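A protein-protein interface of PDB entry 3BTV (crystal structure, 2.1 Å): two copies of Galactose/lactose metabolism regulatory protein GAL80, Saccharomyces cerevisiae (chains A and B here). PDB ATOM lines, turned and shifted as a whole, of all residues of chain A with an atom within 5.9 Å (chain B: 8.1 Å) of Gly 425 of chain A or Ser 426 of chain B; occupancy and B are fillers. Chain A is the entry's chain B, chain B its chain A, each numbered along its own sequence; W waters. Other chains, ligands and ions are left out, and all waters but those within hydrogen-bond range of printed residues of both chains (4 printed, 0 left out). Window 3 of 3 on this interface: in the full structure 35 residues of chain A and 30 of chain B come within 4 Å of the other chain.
The side-chain hydroxyl (OG) of Ser 421 of chain A lies within hydrogen-bond range of the backbone carbonyl oxygen (O) of Ser 426 of chain A (2.7 Å). OD1 of Asn 233 of chain B sits close to O of Ser 426 of chain B, at 3.4 Å. The backbone carbonyl oxygen (O) of Ser 426 of chain B sits at hydrogen-bond distance from the side-chain hydroxyl (OG) of Ser 421 of chain B (3.0 Å). The side-chain amide oxygen of Asn 233 of chain A sits at hydrogen-bond distance from the side-chain hydroxyl of Thr 427 of chain A, at 3.4 Å. The backbone carbonyl oxygen of Ser 426 of chain A lies close to the side-chain amide oxygen of Asn 233 of chain A (3.3 Å). The side-chain amide oxygen of Asn 233 of chain B sits at hydrogen-bond distance from the backbone NH of Thr 427 of chain B, at 3.4 Å.
Asn 233 of chain B touches its own counterpart, Asn 233 of chain A. Asn 233 of chain A touches Thr 427 of chain B, and with the chains exchanged Thr 427 of chain A touches Asn 233 of chain B. Gly 425 of chain A touches Ser 426 of chain B, and with the chains exchanged Ser 426 of chain A touches Gly 425 of chain B. Gly 425 of chain A touches Thr 427 of chain B, and with the chains exchanged Thr 427 of chain A touches Gly 425 of chain B. Positions printed for both chains: 233, 420, 421, 422, 423, 424, 425, 426 and 427. Of the 7 pairs that touch across the chains among the printed residues, 7 have their exchanged pair printed and touching as well.
Gly 425 of chain A touches Ser 426 of chain B. Ser 426 of chain A touches Gly 425 of chain B (CA to O, 3.8 Å).
Of the printed residues of chain B, Asn 233 of chain A touches Asn 233 and Thr 427. Of chain B, only Ser 426 and Thr 427 come within 4 Å of Gly 425 of chain A. Of the printed residues of chain B, Thr 427 of chain A touches Asn 233 (3.3 Å) and Gly 425 (2.9 Å). Printed residues of chain A within 4 Å of Asn 233 of chain B: Asn 233 (2.9 Å) and Thr 427 (3.3 Å). Ser 426 of chain B touches just one residue of chain A: Gly 425 (3.5 Å). Printed residues of chain A within 4 Å of Thr 427 of chain B: Asn 233 and Gly 425. The nearest printed residue of chain A that does not touch Gly 425 of chain B is Gly 425 of chain A (5.0 Å).
The backbone carbonyl oxygen (O) of Gly 425 of chain A sits at hydrogen-bond distance from the backbone NH (N) of Thr 427 of chain B (2.8 Å). OG1 of Thr 427 of chain B is in hydrogen-bond range of OD1 of Asn 233 of chain A (3.4 Å). OD1 of Asn 233 of chain B lies close to OD1 of Asn 233 of chain A, at 2.9 Å. OG1 of Thr 427 of chain A sits at hydrogen-bond distance from OD1 of Asn 233 of chain B. The backbone NH of Thr 427 of chain A is in hydrogen-bond range of the backbone carbonyl oxygen of Gly 425 of chain B, 2.9 Å away.
Of the 9 printed residues of chain A, 4 touch a printed residue of chain B. Along chain B the printed residues that touch a printed residue of chain A span positions 233 to 427. Among the printed residues, 7 pairs touch across the chains.
Water W1 bridges OG1 of Thr 427 of chain B and ND2 of Asn 233 of chain A. Water W3 lies within hydrogen-bond range of the side-chain hydroxyl (OG1) of Thr 427 of chain A (2.6 Å), the backbone carbonyl oxygen (O) of Ala 234 of chain B (3.0 Å) and the side-chain amide nitrogen (ND2) of Asn 233 of chain B (3.2 Å). Water W4 lies within hydrogen-bond range of NH2 of Arg 231 of chain B and O of Met 423 of chain A. Water W2 lies within hydrogen-bond range of the backbone carbonyl oxygen (O) of Gly 425 of chain B (2.9 Å) and the backbone carbonyl oxygen (O) of Thr 427 of chain A (3.1 Å).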
ATOM      1  N   ASN A 233      -8.469 -31.726 -12.738  1.00  0.00           N
ATOM      2  CA  ASN A 233      -9.900 -31.949 -12.818  1.00  0.00           C
ATOM      3  C   ASN A 233     -10.271 -32.216 -14.260  1.00  0.00           C
ATOM      4  O   ASN A 233      -9.800 -31.530 -15.166  1.00  0.00           O
ATOM      5  CB  ASN A 233     -10.685 -30.722 -12.346  1.00  0.00           C
ATOM      6  CG  ASN A 233     -12.173 -31.028 -12.155  1.00  0.00           C
ATOM      7  OD1 ASN A 233     -12.601 -31.433 -11.074  1.00  0.00           O
ATOM      8  ND2 ASN A 233     -12.960 -30.845 -13.211  1.00  0.00           N
ATOM      9  N   LYS A 420     -11.443 -40.881 -13.047  1.00  0.00           N
ATOM     10  CA  LYS A 420     -11.906 -40.796 -11.658  1.00  0.00           C
ATOM     11  C   LYS A 420     -12.466 -39.419 -11.379  1.00  0.00           C
ATOM     12  O   LYS A 420     -13.563 -39.296 -10.838  1.00  0.00           O
ATOM     13  CB  LYS A 420     -10.786 -41.077 -10.656  1.00  0.00           C
ATOM     14  CG  LYS A 420     -10.618 -42.515 -10.245  1.00  0.00           C
ATOM     15  CD  LYS A 420      -9.700 -42.618  -9.036  1.00  0.00           C
ATOM     16  CE  LYS A 420      -8.864 -43.890  -9.096  1.00  0.00           C
ATOM     17  NZ  LYS A 420      -9.663 -45.083  -9.499  1.00  0.00           N
ATOM     18  N   SER A 421     -11.697 -38.391 -11.747  1.00  0.00           N
ATOM     19  CA  SER A 421     -12.092 -37.012 -11.549  1.00  0.00           C
ATOM     20  C   SER A 421     -13.476 -36.728 -12.098  1.00  0.00           C
ATOM     21  O   SER A 421     -14.291 -36.086 -11.446  1.00  0.00           O
ATOM     22  CB  SER A 421     -11.083 -36.058 -12.237  1.00  0.00           C
ATOM     23  OG  SER A 421     -11.552 -34.739 -12.106  1.00  0.00           O
ATOM     24  N   ASN A 422     -13.716 -37.173 -13.324  1.00  0.00           N
ATOM     25  CA  ASN A 422     -15.015 -37.025 -13.954  1.00  0.00           C
ATOM     26  C   ASN A 422     -16.135 -37.740 -13.161  1.00  0.00           C
ATOM     27  O   ASN A 422     -17.207 -37.186 -12.926  1.00  0.00           O
ATOM     28  CB  ASN A 422     -14.959 -37.597 -15.372  1.00  0.00           C
ATOM     29  CG  ASN A 422     -16.283 -37.489 -16.090  1.00  0.00           C
ATOM     30  OD1 ASN A 422     -16.786 -36.395 -16.317  1.00  0.00           O
ATOM     31  ND2 ASN A 422     -16.862 -38.630 -16.448  1.00  0.00           N
ATOM     32  N   MET A 423     -15.881 -38.965 -12.749  1.00  0.00           N
ATOM     33  CA  MET A 423     -16.961 -39.727 -12.123  1.00  0.00           C
ATOM     34  C   MET A 423     -17.265 -39.161 -10.738  1.00  0.00           C
ATOM     35  O   MET A 423     -18.422 -38.902 -10.415  1.00  0.00           O
ATOM     36  CB  MET A 423     -16.644 -41.220 -12.104  1.00  0.00           C
ATOM     37  CG  MET A 423     -16.286 -41.781 -10.745  1.00  0.00           C
ATOM     38  SD  MET A 423     -16.473 -43.577 -10.693  1.00  0.00           S
ATOM     39  CE  MET A 423     -15.476 -44.056 -12.101  1.00  0.00           C
ATOM     40  N   MET A 424     -16.220 -38.900  -9.957  1.00  0.00           N
ATOM     41  CA  MET A 424     -16.359 -38.313  -8.620  1.00  0.00           C
ATOM     42  C   MET A 424     -16.728 -36.837  -8.651  1.00  0.00           C
ATOM     43  O   MET A 424     -17.182 -36.279  -7.654  1.00  0.00           O
ATOM     44  CB  MET A 424     -15.055 -38.461  -7.830  1.00  0.00           C
ATOM     45  CG  MET A 424     -14.621 -39.891  -7.551  1.00  0.00           C
ATOM     46  SD  MET A 424     -13.017 -39.971  -6.717  1.00  0.00           S
ATOM     47  CE  MET A 424     -13.331 -39.053  -5.209  1.00  0.00           C
ATOM     48  N   GLY A 425     -16.517 -36.190  -9.788  1.00  0.00           N
ATOM     49  CA  GLY A 425     -16.692 -34.757  -9.839  1.00  0.00           C
ATOM     50  C   GLY A 425     -15.772 -34.072  -8.840  1.00  0.00           C
ATOM     51  O   GLY A 425     -16.137 -33.065  -8.224  1.00  0.00           O
ATOM     52  N   SER A 426     -14.565 -34.601  -8.677  1.00  0.00           N
ATOM     53  CA  SER A 426     -13.590 -33.936  -7.812  1.00  0.00           C
ATOM     54  C   SER A 426     -12.270 -33.593  -8.495  1.00  0.00           C
ATOM     55  O   SER A 426     -11.842 -34.250  -9.444  1.00  0.00           O
ATOM     56  CB  SER A 426     -13.282 -34.779  -6.578  1.00  0.00           C
ATOM     57  OG  SER A 426     -12.313 -35.760  -6.890  1.00  0.00           O
ATOM     58  N   THR A 427     -11.630 -32.561  -7.966  1.00  0.00           N
ATOM     59  CA  THR A 427     -10.261 -32.238  -8.305  1.00  0.00           C
ATOM     60  C   THR A 427      -9.350 -33.173  -7.524  1.00  0.00           C
ATOM     61  O   THR A 427      -9.389 -33.212  -6.296  1.00  0.00           O
ATOM     62  CB  THR A 427      -9.953 -30.793  -7.924  1.00  0.00           C
ATOM     63  OG1 THR A 427     -10.795 -29.923  -8.685  1.00  0.00           O
ATOM     64  CG2 THR A 427      -8.486 -30.461  -8.189  1.00  0.00           C
ATOM     65  N   ARG B 231     -22.948 -27.414 -14.439  1.00  0.00           N
ATOM     66  CA  ARG B 231     -21.868 -27.807 -13.544  1.00  0.00           C
ATOM     67  C   ARG B 231     -20.624 -26.990 -13.883  1.00  0.00           C
ATOM     68  O   ARG B 231     -20.412 -26.658 -15.034  1.00  0.00           O
ATOM     69  CB  ARG B 231     -21.562 -29.291 -13.688  1.00  0.00           C
ATOM     70  CG  ARG B 231     -22.761 -30.192 -13.353  1.00  0.00           C
ATOM     71  CD  ARG B 231     -22.419 -31.682 -13.402  1.00  0.00           C
ATOM     72  NE  ARG B 231     -21.643 -32.107 -12.242  1.00  0.00           N
ATOM     73  CZ  ARG B 231     -21.627 -33.347 -11.764  1.00  0.00           C
ATOM     74  NH1 ARG B 231     -22.358 -34.292 -12.343  1.00  0.00           N
ATOM     75  NH2 ARG B 231     -20.887 -33.640 -10.702  1.00  0.00           N
ATOM     76  N   ILE B 232     -19.824 -26.655 -12.879  1.00  0.00           N
ATOM     77  CA  ILE B 232     -18.564 -25.939 -13.118  1.00  0.00           C
ATOM     78  C   ILE B 232     -17.446 -26.476 -12.231  1.00  0.00           C
ATOM     79  O   ILE B 232     -17.699 -27.058 -11.170  1.00  0.00           O
ATOM     80  CB  ILE B 232     -18.719 -24.431 -12.864  1.00  0.00           C
ATOM     81  CG1 ILE B 232     -19.137 -24.191 -11.413  1.00  0.00           C
ATOM     82  CG2 ILE B 232     -19.781 -23.841 -13.796  1.00  0.00           C
ATOM     83  CD1 ILE B 232     -18.371 -23.143 -10.691  1.00  0.00           C
ATOM     84  N   ASN B 233     -16.209 -26.302 -12.688  1.00  0.00           N
ATOM     85  CA  ASN B 233     -15.033 -26.472 -11.841  1.00  0.00           C
ATOM     86  C   ASN B 233     -14.049 -25.333 -12.113  1.00  0.00           C
ATOM     87  O   ASN B 233     -13.816 -24.985 -13.256  1.00  0.00           O
ATOM     88  CB  ASN B 233     -14.352 -27.802 -12.136  1.00  0.00           C
ATOM     89  CG  ASN B 233     -13.257 -28.129 -11.139  1.00  0.00           C
ATOM     90  OD1 ASN B 233     -13.499 -28.793 -10.125  1.00  0.00           O
ATOM     91  ND2 ASN B 233     -12.048 -27.657 -11.414  1.00  0.00           N
ATOM     92  N   ALA B 234     -13.469 -24.762 -11.068  1.00  0.00           N
ATOM     93  CA  ALA B 234     -12.497 -23.691 -11.236  1.00  0.00           C
ATOM     94  C   ALA B 234     -11.261 -23.919 -10.417  1.00  0.00           C
ATOM     95  O   ALA B 234     -11.317 -24.508  -9.334  1.00  0.00           O
ATOM     96  CB  ALA B 234     -13.114 -22.348 -10.853  1.00  0.00           C
ATOM     97  N   SER B 417     -19.595 -19.280  -6.602  1.00  0.00           N
ATOM     98  CA  SER B 417     -19.428 -20.720  -6.850  1.00  0.00           C
ATOM     99  C   SER B 417     -18.043 -21.045  -7.442  1.00  0.00           C
ATOM    100  O   SER B 417     -17.464 -22.102  -7.178  1.00  0.00           O
ATOM    101  CB  SER B 417     -20.503 -21.240  -7.803  1.00  0.00           C
ATOM    102  OG  SER B 417     -21.792 -21.094  -7.230  1.00  0.00           O
ATOM    103  N   VAL B 418     -17.527 -20.156  -8.275  1.00  0.00           N
ATOM    104  CA  VAL B 418     -16.170 -20.342  -8.823  1.00  0.00           C
ATOM    105  C   VAL B 418     -15.146 -20.426  -7.700  1.00  0.00           C
ATOM    106  O   VAL B 418     -14.335 -21.346  -7.643  1.00  0.00           O
ATOM    107  CB  VAL B 418     -15.823 -19.182  -9.781  1.00  0.00           C
ATOM    108  CG1 VAL B 418     -14.336 -19.217 -10.187  1.00  0.00           C
ATOM    109  CG2 VAL B 418     -16.720 -19.278 -10.994  1.00  0.00           C
ATOM    110  N   LYS B 420     -15.779 -21.091  -4.551  1.00  0.00           N
ATOM    111  CA  LYS B 420     -16.080 -22.220  -3.665  1.00  0.00           C
ATOM    112  C   LYS B 420     -15.471 -23.478  -4.270  1.00  0.00           C
ATOM    113  O   LYS B 420     -14.834 -24.268  -3.576  1.00  0.00           O
ATOM    114  CB  LYS B 420     -17.593 -22.403  -3.547  1.00  0.00           C
ATOM    115  CG  LYS B 420     -18.236 -21.791  -2.327  1.00  0.00           C
ATOM    116  CD  LYS B 420     -19.760 -21.961  -2.368  1.00  0.00           C
ATOM    117  CE  LYS B 420     -20.178 -23.409  -2.634  1.00  0.00           C
ATOM    118  NZ  LYS B 420     -21.672 -23.622  -2.514  1.00  0.00           N
ATOM    119  N   SER B 421     -15.658 -23.632  -5.582  1.00  0.00           N
ATOM    120  CA  SER B 421     -15.195 -24.799  -6.317  1.00  0.00           C
ATOM    121  C   SER B 421     -13.697 -24.952  -6.148  1.00  0.00           C
ATOM    122  O   SER B 421     -13.187 -26.052  -5.976  1.00  0.00           O
ATOM    123  CB  SER B 421     -15.507 -24.642  -7.806  1.00  0.00           C
ATOM    124  OG  SER B 421     -14.850 -25.647  -8.574  1.00  0.00           O
ATOM    125  N   ASN B 422     -12.996 -23.829  -6.211  1.00  0.00           N
ATOM    126  CA  ASN B 422     -11.550 -23.810  -6.017  1.00  0.00           C
ATOM    127  C   ASN B 422     -11.186 -24.241  -4.593  1.00  0.00           C
ATOM    128  O   ASN B 422     -10.319 -25.083  -4.376  1.00  0.00           O
ATOM    129  CB  ASN B 422     -11.022 -22.396  -6.272  1.00  0.00           C
ATOM    130  CG  ASN B 422      -9.547 -22.299  -6.054  1.00  0.00           C
ATOM    131  OD1 ASN B 422      -8.748 -22.870  -6.804  1.00  0.00           O
ATOM    132  ND2 ASN B 422      -9.167 -21.596  -5.008  1.00  0.00           N
ATOM    133  N   MET B 423     -11.863 -23.641  -3.628  1.00  0.00           N
ATOM    134  CA  MET B 423     -11.678 -23.965  -2.213  1.00  0.00           C
ATOM    135  C   MET B 423     -11.983 -25.438  -1.875  1.00  0.00           C
ATOM    136  O   MET B 423     -11.256 -26.063  -1.109  1.00  0.00           O
ATOM    137  CB  MET B 423     -12.573 -23.056  -1.370  1.00  0.00           C
ATOM    138  CG  MET B 423     -12.408 -23.224   0.128  1.00  0.00           C
ATOM    139  SD  MET B 423     -14.000 -23.198   0.961  1.00  0.00           S
ATOM    140  CE  MET B 423     -14.452 -24.935   0.857  1.00  0.00           C
ATOM    141  N   MET B 424     -13.065 -25.975  -2.426  1.00  0.00           N
ATOM    142  CA  MET B 424     -13.506 -27.329  -2.078  1.00  0.00           C
ATOM    143  C   MET B 424     -12.774 -28.353  -2.919  1.00  0.00           C
ATOM    144  O   MET B 424     -12.674 -29.516  -2.543  1.00  0.00           O
ATOM    145  CB  MET B 424     -15.013 -27.520  -2.313  1.00  0.00           C
ATOM    146  CG  MET B 424     -15.954 -26.645  -1.481  1.00  0.00           C
ATOM    147  SD  MET B 424     -17.655 -26.810  -2.105  1.00  0.00           S
ATOM    148  CE  MET B 424     -17.949 -28.580  -1.881  1.00  0.00           C
ATOM    149  N   GLY B 425     -12.287 -27.927  -4.076  1.00  0.00           N
ATOM    150  CA  GLY B 425     -11.637 -28.853  -4.975  1.00  0.00           C
ATOM    151  C   GLY B 425     -12.641 -29.834  -5.547  1.00  0.00           C
ATOM    152  O   GLY B 425     -12.360 -31.024  -5.673  1.00  0.00           O
ATOM    153  N   SER B 426     -13.824 -29.349  -5.905  1.00  0.00           N
ATOM    154  CA  SER B 426     -14.787 -30.229  -6.554  1.00  0.00           C
ATOM    155  C   SER B 426     -15.600 -29.531  -7.630  1.00  0.00           C
ATOM    156  O   SER B 426     -15.738 -28.318  -7.628  1.00  0.00           O
ATOM    157  CB  SER B 426     -15.716 -30.873  -5.519  1.00  0.00           C
ATOM    158  OG  SER B 426     -16.314 -29.892  -4.706  1.00  0.00           O
ATOM    159  N   THR B 427     -16.138 -30.316  -8.551  1.00  0.00           N
ATOM    160  CA  THR B 427     -17.065 -29.804  -9.543  1.00  0.00           C
ATOM    161  C   THR B 427     -18.395 -29.496  -8.847  1.00  0.00           C
ATOM    162  O   THR B 427     -18.883 -30.288  -8.043  1.00  0.00           O
ATOM    163  CB  THR B 427     -17.258 -30.833 -10.653  1.00  0.00           C
ATOM    164  OG1 THR B 427     -15.978 -31.142 -11.220  1.00  0.00           O
ATOM    165  CG2 THR B 427     -18.190 -30.324 -11.726  1.00  0.00           C
ATOM    166  N   LEU B 428     -18.980 -28.342  -9.139  1.00  0.00           N
ATOM    167  CA  LEU B 428     -20.161 -27.894  -8.382  1.00  0.00           C
ATOM    168  C   LEU B 428     -21.374 -27.858  -9.276  1.00  0.00           C
ATOM    169  O   LEU B 428     -21.282 -27.502 -10.454  1.00  0.00           O
ATOM    170  CB  LEU B 428     -19.906 -26.505  -7.786  1.00  0.00           C
ATOM    171  CG  LEU B 428     -19.639 -26.321  -6.295  1.00  0.00           C
ATOM    172  CD1 LEU B 428     -19.070 -27.562  -5.634  1.00  0.00           C
ATOM    173  CD2 LEU B 428     -18.769 -25.089  -6.041  1.00  0.00           C
ATOM    174  N   ASN B 429     -22.503 -28.280  -8.725  1.00  0.00           N
ATOM    175  CA  ASN B 429     -23.790 -28.154  -9.386  1.00  0.00           C
ATOM    176  C   ASN B 429     -24.301 -26.725  -9.190  1.00  0.00           C
ATOM    177  O   ASN B 429     -24.611 -26.323  -8.069  1.00  0.00           O
ATOM    178  CB  ASN B 429     -24.797 -29.154  -8.744  1.00  0.00           C
ATOM    179  CG  ASN B 429     -26.179 -29.071  -9.363  1.00  0.00           C
ATOM    180  OD1 ASN B 429     -26.390 -28.361 -10.349  1.00  0.00           O
ATOM    181  ND2 ASN B 429     -27.132 -29.803  -8.790  1.00  0.00           N
HETATM  182  O   HOH W   1     -15.329 -33.040 -12.859  1.00  0.00           O
HETATM  183  O   HOH W   2     -10.543 -32.186  -3.664  1.00  0.00           O
HETATM  184  O   HOH W   3     -10.946 -27.300  -8.406  1.00  0.00           O
HETATM  185  O   HOH W   4     -20.849 -36.511 -10.179  1.00  0.00           O
